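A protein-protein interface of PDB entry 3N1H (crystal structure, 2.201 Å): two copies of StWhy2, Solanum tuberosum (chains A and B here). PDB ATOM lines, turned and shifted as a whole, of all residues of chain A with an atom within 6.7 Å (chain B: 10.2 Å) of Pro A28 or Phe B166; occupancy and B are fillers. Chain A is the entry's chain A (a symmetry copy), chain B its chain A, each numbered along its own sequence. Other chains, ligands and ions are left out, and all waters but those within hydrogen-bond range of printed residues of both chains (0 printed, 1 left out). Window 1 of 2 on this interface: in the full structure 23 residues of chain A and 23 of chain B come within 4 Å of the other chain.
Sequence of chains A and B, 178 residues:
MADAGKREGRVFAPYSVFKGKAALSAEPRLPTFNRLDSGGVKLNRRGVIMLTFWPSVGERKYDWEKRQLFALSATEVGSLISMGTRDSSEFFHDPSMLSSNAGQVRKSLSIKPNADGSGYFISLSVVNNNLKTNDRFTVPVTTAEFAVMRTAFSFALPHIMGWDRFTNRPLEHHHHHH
Hydrophobic or aromatic side chains of chain A within 4 Å of the printed part of chain B: Val A11, Phe A12, Ala A13, Pro A28, Leu A30, Ala A152, Phe A155 and His A159.
Of the 17 printed residues of chain B, 11 touch a printed residue of chain A.
Hydrophobic or aromatic side chains of chain B within 4 Å of the printed part of chain A: Val B41, Leu B43, Pro B158, Met B161, Trp B163 and Phe B166.
Among the printed residues, no Asp or Glu carboxylate lies within 4 Å of a Lys or Arg side-chain nitrogen of the other chain.
2 positions are printed for both chains.
Of the 28 pairs that touch across the chains among the printed residues, none has its exchanged pair printed and touching as well.
Among the printed residues, pairs that only touch across the chains: Arg A10 with Gly B40, Val A11 with Val B41, Val A11 with Arg B165, Val A11 with Phe B166, Phe A12 with Lys B42, Ala A13 with Met B161, Ala A13 with Phe B166, Ala A26 with Trp B163, Glu A27 with Trp B163, Glu A27 with Phe B166, Pro A28 with Trp B163, Pro A28 with Phe B166, Leu A30 with Phe B166, Leu A30 with Thr B167, Leu A30 with Asn B168, Ala A152 with Met B161, Ala A152 with Trp B163, Phe A155 with Pro B158, Phe A155 with Trp B163, His A159 with Phe B166, His A159 with Thr B167 and Asp A164 with Thr B167.
Of the printed residues of chain B, Arg A10 touches Gly B40 and Val B41.
Glu A27 touches two residues of chain B.
Pro A28 touches just these residues of chain B: Trp B163 (3.5 Å) and Phe B166 (3.6 Å).
Of the printed residues of chain B, Ala A152 touches Met B161 (3.6 Å) and Trp B163 (3.5 Å).
Ala A156 touches none of the printed residues of chain B.
Of the printed residues of chain B, His A159 touches Phe B166, Thr B167 and Asn B168.
Printed residues of chain A within 4 Å of Gly B40: Arg A10.
Of the printed residues of chain A, Lys B42 touches Phe A12.
Of the printed residues of chain A, Phe B166 touches Val A11, Ala A13, Glu A27, Pro A28, Leu A30 and His A159.
The nearest residue of chain A that does not touch Phe B166 is Phe A12 (4.6 Å).
The nearest printed residue of chain B that does not touch Arg A10 is Lys B42 (5.9 Å).
O of Arg A10 sits at hydrogen-bond distance from N of Val B41 (3.1 Å).
The backbone carbonyl oxygen (O) of Val B41 sits at hydrogen-bond distance from the backbone NH (N) of Phe A12, 2.9 Å away.
N of Leu B43 sits at hydrogen-bond distance from O of Phe A12 (2.9 Å).
The indole nitrogen of Trp B163 lies within hydrogen-bond range of the backbone carbonyl oxygen of Ala A13.
The backbone carbonyl oxygen of His A159 lies within hydrogen-bond range of the side-chain amide nitrogen of Asn B168 (2.9 Å).
ND2 of Asn B168 is in hydrogen-bond range of OD1 of Asp A164, 2.6 Å away.
The backbone carbonyl oxygen (O) of Pro B158 sits at hydrogen-bond distance from the backbone NH (N) of Trp B163.
N of Ala A13 lies within hydrogen-bond range of OE2 of Glu A27 (2.6 Å).
O of Glu A27 lies within hydrogen-bond range of N of Met A50, 2.9 Å away.
ND1 of His A159 sits at hydrogen-bond distance from OD2 of Asp A164.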
ATOM      1  N   ARG A  10     -27.745 -27.694   7.476  1.00  0.00           N
ATOM      2  CA  ARG A  10     -26.728 -28.520   8.115  1.00  0.00           C
ATOM      3  C   ARG A  10     -25.528 -27.664   8.524  1.00  0.00           C
ATOM      4  O   ARG A  10     -25.465 -26.471   8.209  1.00  0.00           O
ATOM      5  CB  ARG A  10     -26.269 -29.668   7.201  1.00  0.00           C
ATOM      6  CG  ARG A  10     -27.150 -29.971   5.979  1.00  0.00           C
ATOM      7  CD  ARG A  10     -26.503 -29.430   4.692  1.00  0.00           C
ATOM      8  NE  ARG A  10     -26.915 -30.142   3.482  1.00  0.00           N
ATOM      9  CZ  ARG A  10     -26.164 -30.251   2.386  1.00  0.00           C
ATOM     10  NH1 ARG A  10     -24.947 -29.708   2.340  1.00  0.00           N
ATOM     11  NH2 ARG A  10     -26.626 -30.916   1.333  1.00  0.00           N
ATOM     12  N   VAL A  11     -24.593 -28.274   9.247  1.00  0.00           N
ATOM     13  CA  VAL A  11     -23.326 -27.643   9.591  1.00  0.00           C
ATOM     14  C   VAL A  11     -22.239 -28.688   9.452  1.00  0.00           C
ATOM     15  O   VAL A  11     -22.385 -29.828   9.911  1.00  0.00           O
ATOM     16  CB  VAL A  11     -23.301 -27.089  11.034  1.00  0.00           C
ATOM     17  CG1 VAL A  11     -21.851 -26.763  11.456  1.00  0.00           C
ATOM     18  CG2 VAL A  11     -24.227 -25.880  11.184  1.00  0.00           C
ATOM     19  N   PHE A  12     -21.151 -28.278   8.804  1.00  0.00           N
ATOM     20  CA  PHE A  12     -19.984 -29.110   8.575  1.00  0.00           C
ATOM     21  C   PHE A  12     -18.759 -28.461   9.211  1.00  0.00           C
ATOM     22  O   PHE A  12     -18.266 -27.449   8.718  1.00  0.00           O
ATOM     23  CB  PHE A  12     -19.773 -29.299   7.072  1.00  0.00           C
ATOM     24  CG  PHE A  12     -20.942 -29.970   6.390  1.00  0.00           C
ATOM     25  CD1 PHE A  12     -21.889 -29.221   5.690  1.00  0.00           C
ATOM     26  CD2 PHE A  12     -21.118 -31.350   6.485  1.00  0.00           C
ATOM     27  CE1 PHE A  12     -22.973 -29.833   5.087  1.00  0.00           C
ATOM     28  CE2 PHE A  12     -22.194 -31.968   5.878  1.00  0.00           C
ATOM     29  CZ  PHE A  12     -23.129 -31.208   5.181  1.00  0.00           C
ATOM     30  N   ALA A  13     -18.266 -29.042  10.304  1.00  0.00           N
ATOM     31  CA  ALA A  13     -17.106 -28.492  10.955  1.00  0.00           C
ATOM     32  C   ALA A  13     -16.301 -29.563  11.717  1.00  0.00           C
ATOM     33  O   ALA A  13     -16.097 -29.484  12.924  1.00  0.00           O
ATOM     34  CB  ALA A  13     -17.519 -27.361  11.833  1.00  0.00           C
ATOM     35  N   PRO A  14     -15.799 -30.555  10.979  1.00  0.00           N
ATOM     36  CA  PRO A  14     -15.162 -31.741  11.559  1.00  0.00           C
ATOM     37  C   PRO A  14     -13.847 -31.349  12.210  1.00  0.00           C
ATOM     38  O   PRO A  14     -13.257 -30.374  11.770  1.00  0.00           O
ATOM     39  CB  PRO A  14     -14.886 -32.622  10.330  1.00  0.00           C
ATOM     40  CG  PRO A  14     -14.672 -31.586   9.208  1.00  0.00           C
ATOM     41  CD  PRO A  14     -15.740 -30.549   9.502  1.00  0.00           C
ATOM     42  N   ALA A  26     -13.841 -36.211  13.288  1.00  0.00           N
ATOM     43  CA  ALA A  26     -14.940 -36.373  14.243  1.00  0.00           C
ATOM     44  C   ALA A  26     -15.851 -35.174  14.148  1.00  0.00           C
ATOM     45  O   ALA A  26     -15.374 -34.029  14.075  1.00  0.00           O
ATOM     46  CB  ALA A  26     -14.407 -36.468  15.669  1.00  0.00           C
ATOM     47  N   GLU A  27     -17.149 -35.433  14.217  1.00  0.00           N
ATOM     48  CA  GLU A  27     -18.129 -34.372  14.177  1.00  0.00           C
ATOM     49  C   GLU A  27     -19.397 -34.784  14.943  1.00  0.00           C
ATOM     50  O   GLU A  27     -19.832 -35.920  14.831  1.00  0.00           O
ATOM     51  CB  GLU A  27     -18.482 -34.135  12.722  1.00  0.00           C
ATOM     52  CG  GLU A  27     -18.986 -32.746  12.406  1.00  0.00           C
ATOM     53  CD  GLU A  27     -19.267 -32.585  10.913  1.00  0.00           C
ATOM     54  OE1 GLU A  27     -19.823 -33.543  10.328  1.00  0.00           O
ATOM     55  OE2 GLU A  27     -18.928 -31.523  10.328  1.00  0.00           O
ATOM     56  N   PRO A  28     -19.994 -33.866  15.716  1.00  0.00           N
ATOM     57  CA  PRO A  28     -21.215 -34.241  16.426  1.00  0.00           C
ATOM     58  C   PRO A  28     -22.361 -34.360  15.442  1.00  0.00           C
ATOM     59  O   PRO A  28     -22.381 -33.693  14.417  1.00  0.00           O
ATOM     60  CB  PRO A  28     -21.462 -33.048  17.375  1.00  0.00           C
ATOM     61  CG  PRO A  28     -20.182 -32.244  17.395  1.00  0.00           C
ATOM     62  CD  PRO A  28     -19.568 -32.484  16.035  1.00  0.00           C
ATOM     63  N   ARG A  29     -23.305 -35.222  15.744  1.00  0.00           N
ATOM     64  CA  ARG A  29     -24.544 -35.288  15.010  1.00  0.00           C
ATOM     65  C   ARG A  29     -25.669 -35.140  16.045  1.00  0.00           C
ATOM     66  O   ARG A  29     -25.806 -35.989  16.924  1.00  0.00           O
ATOM     67  CB  ARG A  29     -24.656 -36.636  14.291  1.00  0.00           C
ATOM     68  CG  ARG A  29     -25.869 -36.727  13.373  1.00  0.00           C
ATOM     69  CD  ARG A  29     -26.175 -38.144  12.947  1.00  0.00           C
ATOM     70  NE  ARG A  29     -27.008 -38.820  13.936  1.00  0.00           N
ATOM     71  CZ  ARG A  29     -27.106 -40.138  14.088  1.00  0.00           C
ATOM     72  NH1 ARG A  29     -26.449 -40.970  13.290  1.00  0.00           N
ATOM     73  NH2 ARG A  29     -27.883 -40.622  15.045  1.00  0.00           N
ATOM     74  N   LEU A  30     -26.453 -34.060  15.943  1.00  0.00           N
ATOM     75  CA  LEU A  30     -27.497 -33.713  16.924  1.00  0.00           C
ATOM     76  C   LEU A  30     -28.568 -34.762  16.918  1.00  0.00           C
ATOM     77  O   LEU A  30     -28.719 -35.495  15.928  1.00  0.00           O
ATOM     78  CB  LEU A  30     -28.128 -32.351  16.625  1.00  0.00           C
ATOM     79  CG  LEU A  30     -27.117 -31.214  16.724  1.00  0.00           C
ATOM     80  CD1 LEU A  30     -27.658 -29.914  16.125  1.00  0.00           C
ATOM     81  CD2 LEU A  30     -26.684 -31.018  18.165  1.00  0.00           C
ATOM     82  N   VAL A  48     -25.041 -38.648  18.375  1.00  0.00           N
ATOM     83  CA  VAL A  48     -23.799 -39.385  18.488  1.00  0.00           C
ATOM     84  C   VAL A  48     -22.630 -38.461  18.153  1.00  0.00           C
ATOM     85  O   VAL A  48     -22.813 -37.345  17.636  1.00  0.00           O
ATOM     86  CB  VAL A  48     -23.767 -40.602  17.508  1.00  0.00           C
ATOM     87  CG1 VAL A  48     -24.948 -41.526  17.739  1.00  0.00           C
ATOM     88  CG2 VAL A  48     -23.726 -40.130  16.056  1.00  0.00           C
ATOM     89  N   ILE A  49     -21.419 -38.917  18.434  1.00  0.00           N
ATOM     90  CA  ILE A  49     -20.285 -38.277  17.814  1.00  0.00           C
ATOM     91  C   ILE A  49     -19.822 -39.197  16.675  1.00  0.00           C
ATOM     92  O   ILE A  49     -19.417 -40.347  16.908  1.00  0.00           O
ATOM     93  CB  ILE A  49     -19.181 -38.019  18.816  1.00  0.00           C
ATOM     94  CG1 ILE A  49     -19.598 -36.895  19.777  1.00  0.00           C
ATOM     95  CG2 ILE A  49     -17.895 -37.664  18.073  1.00  0.00           C
ATOM     96  CD1 ILE A  49     -18.529 -36.488  20.682  1.00  0.00           C
ATOM     97  N   MET A  50     -19.925 -38.718  15.446  1.00  0.00           N
ATOM     98  CA  MET A  50     -19.586 -39.541  14.284  1.00  0.00           C
ATOM     99  C   MET A  50     -18.117 -39.476  13.958  1.00  0.00           C
ATOM    100  O   MET A  50     -17.591 -38.397  13.762  1.00  0.00           O
ATOM    101  CB  MET A  50     -20.354 -39.071  13.061  1.00  0.00           C
ATOM    102  CG  MET A  50     -20.165 -39.985  11.850  1.00  0.00           C
ATOM    103  SD  MET A  50     -20.839 -41.662  12.129  1.00  0.00           S
ATOM    104  CE  MET A  50     -22.597 -41.324  12.249  1.00  0.00           C
ATOM    105  N   ALA A 152     -13.521 -31.322  23.246  1.00  0.00           N
ATOM    106  CA  ALA A 152     -14.593 -31.068  22.302  1.00  0.00           C
ATOM    107  C   ALA A 152     -15.727 -32.099  22.474  1.00  0.00           C
ATOM    108  O   ALA A 152     -16.904 -31.742  22.342  1.00  0.00           O
ATOM    109  CB  ALA A 152     -14.077 -30.992  20.828  1.00  0.00           C
ATOM    110  N   PHE A 155     -17.655 -31.117  25.587  1.00  0.00           N
ATOM    111  CA  PHE A 155     -18.526 -29.972  25.250  1.00  0.00           C
ATOM    112  C   PHE A 155     -19.741 -30.456  24.445  1.00  0.00           C
ATOM    113  O   PHE A 155     -20.846 -29.974  24.619  1.00  0.00           O
ATOM    114  CB  PHE A 155     -17.760 -28.911  24.426  1.00  0.00           C
ATOM    115  CG  PHE A 155     -18.675 -27.912  23.682  1.00  0.00           C
ATOM    116  CD1 PHE A 155     -18.989 -26.664  24.234  1.00  0.00           C
ATOM    117  CD2 PHE A 155     -19.229 -28.225  22.440  1.00  0.00           C
ATOM    118  CE1 PHE A 155     -19.854 -25.749  23.560  1.00  0.00           C
ATOM    119  CE2 PHE A 155     -20.073 -27.324  21.779  1.00  0.00           C
ATOM    120  CZ  PHE A 155     -20.391 -26.084  22.341  1.00  0.00           C
ATOM    121  N   ALA A 156     -19.527 -31.408  23.533  1.00  0.00           N
ATOM    122  CA  ALA A 156     -20.611 -31.868  22.657  1.00  0.00           C
ATOM    123  C   ALA A 156     -21.596 -32.778  23.386  1.00  0.00           C
ATOM    124  O   ALA A 156     -22.767 -32.830  23.015  1.00  0.00           O
ATOM    125  CB  ALA A 156     -20.055 -32.572  21.388  1.00  0.00           C
ATOM    126  N   HIS A 159     -25.029 -31.702  24.207  1.00  0.00           N
ATOM    127  CA  HIS A 159     -25.768 -31.394  22.972  1.00  0.00           C
ATOM    128  C   HIS A 159     -26.302 -32.644  22.293  1.00  0.00           C
ATOM    129  O   HIS A 159     -27.468 -32.699  21.910  1.00  0.00           O
ATOM    130  CB  HIS A 159     -24.914 -30.556  22.006  1.00  0.00           C
ATOM    131  CG  HIS A 159     -24.503 -29.224  22.583  1.00  0.00           C
ATOM    132  ND1 HIS A 159     -25.306 -28.105  22.509  1.00  0.00           N
ATOM    133  CD2 HIS A 159     -23.407 -28.854  23.284  1.00  0.00           C
ATOM    134  CE1 HIS A 159     -24.707 -27.098  23.122  1.00  0.00           C
ATOM    135  NE2 HIS A 159     -23.554 -27.525  23.605  1.00  0.00           N
ATOM    136  N   ILE A 160     -25.467 -33.679  22.191  1.00  0.00           N
ATOM    137  CA  ILE A 160     -25.916 -34.890  21.530  1.00  0.00           C
ATOM    138  C   ILE A 160     -26.929 -35.602  22.405  1.00  0.00           C
ATOM    139  O   ILE A 160     -27.711 -36.392  21.895  1.00  0.00           O
ATOM    140  CB  ILE A 160     -24.764 -35.819  21.060  1.00  0.00           C
ATOM    141  CG1 ILE A 160     -23.956 -36.332  22.263  1.00  0.00           C
ATOM    142  CG2 ILE A 160     -23.857 -35.045  20.072  1.00  0.00           C
ATOM    143  CD1 ILE A 160     -23.119 -37.558  21.974  1.00  0.00           C
ATOM    144  N   ASP A 164     -29.149 -29.446  25.963  1.00  0.00           N
ATOM    145  CA  ASP A 164     -29.031 -28.003  25.657  1.00  0.00           C
ATOM    146  C   ASP A 164     -30.376 -27.327  25.391  1.00  0.00           C
ATOM    147  O   ASP A 164     -30.459 -26.109  25.346  1.00  0.00           O
ATOM    148  CB  ASP A 164     -28.095 -27.736  24.467  1.00  0.00           C
ATOM    149  CG  ASP A 164     -28.524 -28.487  23.165  1.00  0.00           C
ATOM    150  OD1 ASP A 164     -29.276 -29.481  23.226  1.00  0.00           O
ATOM    151  OD2 ASP A 164     -28.082 -28.085  22.064  1.00  0.00           O
ATOM    152  N   PRO B  31     -13.708 -19.045  13.650  1.00  0.00           N
ATOM    153  CA  PRO B  31     -13.468 -19.548  12.298  1.00  0.00           C
ATOM    154  C   PRO B  31     -14.497 -18.884  11.418  1.00  0.00           C
ATOM    155  O   PRO B  31     -15.490 -18.374  11.933  1.00  0.00           O
ATOM    156  CB  PRO B  31     -13.828 -21.026  12.403  1.00  0.00           C
ATOM    157  CG  PRO B  31     -14.901 -21.053  13.451  1.00  0.00           C
ATOM    158  CD  PRO B  31     -14.531 -19.969  14.444  1.00  0.00           C
ATOM    159  N   PHE B  33     -17.060 -19.330   7.972  1.00  0.00           N
ATOM    160  CA  PHE B  33     -17.793 -20.337   7.245  1.00  0.00           C
ATOM    161  C   PHE B  33     -18.183 -19.755   5.883  1.00  0.00           C
ATOM    162  O   PHE B  33     -18.357 -18.539   5.730  1.00  0.00           O
ATOM    163  CB  PHE B  33     -19.056 -20.723   7.994  1.00  0.00           C
ATOM    164  CG  PHE B  33     -18.817 -21.483   9.250  1.00  0.00           C
ATOM    165  CD1 PHE B  33     -18.178 -20.899  10.312  1.00  0.00           C
ATOM    166  CD2 PHE B  33     -19.278 -22.778   9.386  1.00  0.00           C
ATOM    167  CE1 PHE B  33     -17.966 -21.610  11.484  1.00  0.00           C
ATOM    168  CE2 PHE B  33     -19.082 -23.480  10.547  1.00  0.00           C
ATOM    169  CZ  PHE B  33     -18.421 -22.891  11.605  1.00  0.00           C
ATOM    170  N   GLY B  40     -27.129 -24.657   4.455  1.00  0.00           N
ATOM    171  CA  GLY B  40     -26.281 -24.759   5.621  1.00  0.00           C
ATOM    172  C   GLY B  40     -24.861 -24.295   5.336  1.00  0.00           C
ATOM    173  O   GLY B  40     -24.574 -23.732   4.274  1.00  0.00           O
ATOM    174  N   VAL B  41     -23.968 -24.550   6.288  1.00  0.00           N
ATOM    175  CA  VAL B  41     -22.651 -23.934   6.298  1.00  0.00           C
ATOM    176  C   VAL B  41     -21.488 -24.923   6.439  1.00  0.00           C
ATOM    177  O   VAL B  41     -21.634 -26.005   7.011  1.00  0.00           O
ATOM    178  CB  VAL B  41     -22.573 -22.841   7.381  1.00  0.00           C
ATOM    179  CG1 VAL B  41     -23.543 -21.719   7.050  1.00  0.00           C
ATOM    180  CG2 VAL B  41     -22.891 -23.407   8.770  1.00  0.00           C
ATOM    181  N   LYS B  42     -20.342 -24.546   5.883  1.00  0.00           N
ATOM    182  CA  LYS B  42     -19.124 -25.337   5.964  1.00  0.00           C
ATOM    183  C   LYS B  42     -17.955 -24.484   6.485  1.00  0.00           C
ATOM    184  O   LYS B  42     -17.675 -23.413   5.942  1.00  0.00           O
ATOM    185  CB  LYS B  42     -18.767 -25.915   4.596  1.00  0.00           C
ATOM    186  CG  LYS B  42     -17.366 -26.517   4.554  1.00  0.00           C
ATOM    187  CD  LYS B  42     -17.274 -27.700   3.591  1.00  0.00           C
ATOM    188  CE  LYS B  42     -15.806 -28.136   3.364  1.00  0.00           C
ATOM    189  NZ  LYS B  42     -15.673 -29.369   2.496  1.00  0.00           N
ATOM    190  N   LEU B  43     -17.277 -24.949   7.532  1.00  0.00           N
ATOM    191  CA  LEU B  43     -16.137 -24.197   8.055  1.00  0.00           C
ATOM    192  C   LEU B  43     -15.119 -24.009   6.937  1.00  0.00           C
ATOM    193  O   LEU B  43     -14.797 -24.955   6.224  1.00  0.00           O
ATOM    194  CB  LEU B  43     -15.482 -24.899   9.256  1.00  0.00           C
ATOM    195  CG  LEU B  43     -14.495 -24.050  10.069  1.00  0.00           C
ATOM    196  CD1 LEU B  43     -14.292 -24.634  11.444  1.00  0.00           C
ATOM    197  CD2 LEU B  43     -13.163 -23.915   9.368  1.00  0.00           C
ATOM    198  N   PRO B 158     -14.221 -25.257  21.765  1.00  0.00           N
ATOM    199  CA  PRO B 158     -15.296 -25.697  20.882  1.00  0.00           C
ATOM    200  C   PRO B 158     -15.704 -24.593  19.908  1.00  0.00           C
ATOM    201  O   PRO B 158     -16.137 -24.923  18.794  1.00  0.00           O
ATOM    202  CB  PRO B 158     -16.455 -25.979  21.842  1.00  0.00           C
ATOM    203  CG  PRO B 158     -15.811 -26.190  23.193  1.00  0.00           C
ATOM    204  CD  PRO B 158     -14.516 -25.471  23.196  1.00  0.00           C
ATOM    205  N   HIS B 159     -15.588 -23.325  20.311  1.00  0.00           N
ATOM    206  CA  HIS B 159     -15.983 -22.191  19.460  1.00  0.00           C
ATOM    207  C   HIS B 159     -15.021 -21.976  18.304  1.00  0.00           C
ATOM    208  O   HIS B 159     -15.443 -21.818  17.160  1.00  0.00           O
ATOM    209  CB  HIS B 159     -16.155 -20.907  20.289  1.00  0.00           C
ATOM    210  CG  HIS B 159     -17.227 -21.022  21.344  1.00  0.00           C
ATOM    211  ND1 HIS B 159     -18.558 -20.777  21.079  1.00  0.00           N
ATOM    212  CD2 HIS B 159     -17.166 -21.407  22.639  1.00  0.00           C
ATOM    213  CE1 HIS B 159     -19.266 -20.985  22.175  1.00  0.00           C
ATOM    214  NE2 HIS B 159     -18.448 -21.371  23.138  1.00  0.00           N
ATOM    215  N   MET B 161     -13.269 -24.134  17.052  1.00  0.00           N
ATOM    216  CA  MET B 161     -13.407 -25.333  16.225  1.00  0.00           C
ATOM    217  C   MET B 161     -14.683 -25.257  15.401  1.00  0.00           C
ATOM    218  O   MET B 161     -14.872 -26.038  14.502  1.00  0.00           O
ATOM    219  CB  MET B 161     -13.449 -26.615  17.082  1.00  0.00           C
ATOM    220  CG  MET B 161     -12.119 -27.022  17.716  1.00  0.00           C
ATOM    221  SD  MET B 161     -12.406 -28.345  18.923  1.00  0.00           S
ATOM    222  CE  MET B 161     -12.666 -29.696  17.757  1.00  0.00           C
ATOM    223  N   GLY B 162     -15.572 -24.334  15.726  1.00  0.00           N
ATOM    224  CA  GLY B 162     -16.860 -24.277  15.048  1.00  0.00           C
ATOM    225  C   GLY B 162     -17.933 -25.237  15.554  1.00  0.00           C
ATOM    226  O   GLY B 162     -19.038 -25.303  15.013  1.00  0.00           O
ATOM    227  N   TRP B 163     -17.618 -25.988  16.601  1.00  0.00           N
ATOM    228  CA  TRP B 163     -18.559 -26.961  17.102  1.00  0.00           C
ATOM    229  C   TRP B 163     -19.774 -26.350  17.806  1.00  0.00           C
ATOM    230  O   TRP B 163     -20.709 -27.075  18.090  1.00  0.00           O
ATOM    231  CB  TRP B 163     -17.839 -27.968  18.008  1.00  0.00           C
ATOM    232  CG  TRP B 163     -17.143 -29.042  17.230  1.00  0.00           C
ATOM    233  CD1 TRP B 163     -16.598 -28.927  15.986  1.00  0.00           C
ATOM    234  CD2 TRP B 163     -16.913 -30.393  17.654  1.00  0.00           C
ATOM    235  NE1 TRP B 163     -16.044 -30.132  15.599  1.00  0.00           N
ATOM    236  CE2 TRP B 163     -16.220 -31.047  16.608  1.00  0.00           C
ATOM    237  CE3 TRP B 163     -17.212 -31.109  18.818  1.00  0.00           C
ATOM    238  CZ2 TRP B 163     -15.818 -32.384  16.697  1.00  0.00           C
ATOM    239  CZ3 TRP B 163     -16.827 -32.449  18.900  1.00  0.00           C
ATOM    240  CH2 TRP B 163     -16.127 -33.069  17.839  1.00  0.00           C
ATOM    241  N   ASP B 164     -19.748 -25.045  18.101  1.00  0.00           N
ATOM    242  CA  ASP B 164     -20.898 -24.341  18.710  1.00  0.00           C
ATOM    243  C   ASP B 164     -22.059 -24.124  17.738  1.00  0.00           C
ATOM    244  O   ASP B 164     -23.150 -23.762  18.150  1.00  0.00           O
ATOM    245  CB  ASP B 164     -20.496 -22.988  19.317  1.00  0.00           C
ATOM    246  CG  ASP B 164     -19.814 -22.029  18.288  1.00  0.00           C
ATOM    247  OD1 ASP B 164     -19.304 -22.481  17.243  1.00  0.00           O
ATOM    248  OD2 ASP B 164     -19.772 -20.803  18.543  1.00  0.00           O
ATOM    249  N   ARG B 165     -21.812 -24.327  16.449  1.00  0.00           N
ATOM    250  CA  ARG B 165     -22.897 -24.314  15.463  1.00  0.00           C
ATOM    251  C   ARG B 165     -23.765 -25.551  15.605  1.00  0.00           C
ATOM    252  O   ARG B 165     -24.889 -25.570  15.140  1.00  0.00           O
ATOM    253  CB  ARG B 165     -22.350 -24.299  14.039  1.00  0.00           C
ATOM    254  CG  ARG B 165     -21.757 -22.992  13.600  1.00  0.00           C
ATOM    255  CD  ARG B 165     -22.774 -21.867  13.616  1.00  0.00           C
ATOM    256  NE  ARG B 165     -22.342 -20.802  12.714  1.00  0.00           N
ATOM    257  CZ  ARG B 165     -22.956 -20.483  11.575  1.00  0.00           C
ATOM    258  NH1 ARG B 165     -24.060 -21.127  11.219  1.00  0.00           N
ATOM    259  NH2 ARG B 165     -22.478 -19.511  10.805  1.00  0.00           N
ATOM    260  N   PHE B 166     -23.224 -26.599  16.222  1.00  0.00           N
ATOM    261  CA  PHE B 166     -24.001 -27.816  16.507  1.00  0.00           C
ATOM    262  C   PHE B 166     -24.788 -27.633  17.805  1.00  0.00           C
ATOM    263  O   PHE B 166     -24.453 -28.216  18.849  1.00  0.00           O
ATOM    264  CB  PHE B 166     -23.091 -29.064  16.612  1.00  0.00           C
ATOM    265  CG  PHE B 166     -22.328 -29.388  15.342  1.00  0.00           C
ATOM    266  CD1 PHE B 166     -20.945 -29.196  15.267  1.00  0.00           C
ATOM    267  CD2 PHE B 166     -22.990 -29.885  14.232  1.00  0.00           C
ATOM    268  CE1 PHE B 166     -20.254 -29.501  14.107  1.00  0.00           C
ATOM    269  CE2 PHE B 166     -22.304 -30.198  13.091  1.00  0.00           C
ATOM    270  CZ  PHE B 166     -20.939 -29.992  13.022  1.00  0.00           C
ATOM    271  N   THR B 167     -25.823 -26.804  17.752  1.00  0.00           N
ATOM    272  CA  THR B 167     -26.714 -26.647  18.907  1.00  0.00           C
ATOM    273  C   THR B 167     -28.177 -26.899  18.500  1.00  0.00           C
ATOM    274  O   THR B 167     -28.619 -26.530  17.383  1.00  0.00           O
ATOM    275  CB  THR B 167     -26.553 -25.270  19.624  1.00  0.00           C
ATOM    276  OG1 THR B 167     -26.743 -24.211  18.671  1.00  0.00           O
ATOM    277  CG2 THR B 167     -25.157 -25.134  20.278  1.00  0.00           C
ATOM    278  N   ASN B 168     -28.897 -27.562  19.412  1.00  0.00           N
ATOM    279  CA  ASN B 168     -30.295 -27.925  19.200  1.00  0.00           C
ATOM    280  C   ASN B 168     -31.187 -26.691  19.170  1.00  0.00           C
ATOM    281  O   ASN B 168     -32.404 -26.829  19.092  1.00  0.00           O
ATOM    282  CB  ASN B 168     -30.792 -28.948  20.246  1.00  0.00           C
ATOM    283  CG  ASN B 168     -30.228 -30.346  20.011  1.00  0.00           C
ATOM    284  OD1 ASN B 168     -30.432 -30.917  18.936  1.00  0.00           O
ATOM    285  ND2 ASN B 168     -29.492 -30.900  21.008  1.00  0.00           N
ATOM    286  N   ARG B 169     -30.560 -25.506  19.218  1.00  0.00           N
ATOM    287  CA  ARG B 169     -31.202 -24.175  19.084  1.00  0.00           C
ATOM    288  C   ARG B 169     -32.445 -24.122  19.933  1.00  0.00           C
ATOM    289  O   ARG B 169     -33.092 -23.090  20.159  1.00  0.00           O
ATOM    290  CB  ARG B 169     -31.571 -23.862  17.620  1.00  0.00           C
ATOM    291  CG  ARG B 169     -33.085 -23.804  17.352  1.00  0.00           C
ATOM    292  CD  ARG B 169     -33.735 -25.188  17.208  1.00  0.00           C
ATOM    293  NE  ARG B 169     -33.895 -25.581  15.807  1.00  0.00           N
ATOM    294  CZ  ARG B 169     -34.801 -26.455  15.375  1.00  0.00           C
ATOM    295  NH1 ARG B 169     -35.636 -27.035  16.236  1.00  0.00           N
ATOM    296  NH2 ARG B 169     -34.880 -26.747  14.082  1.00  0.00           N
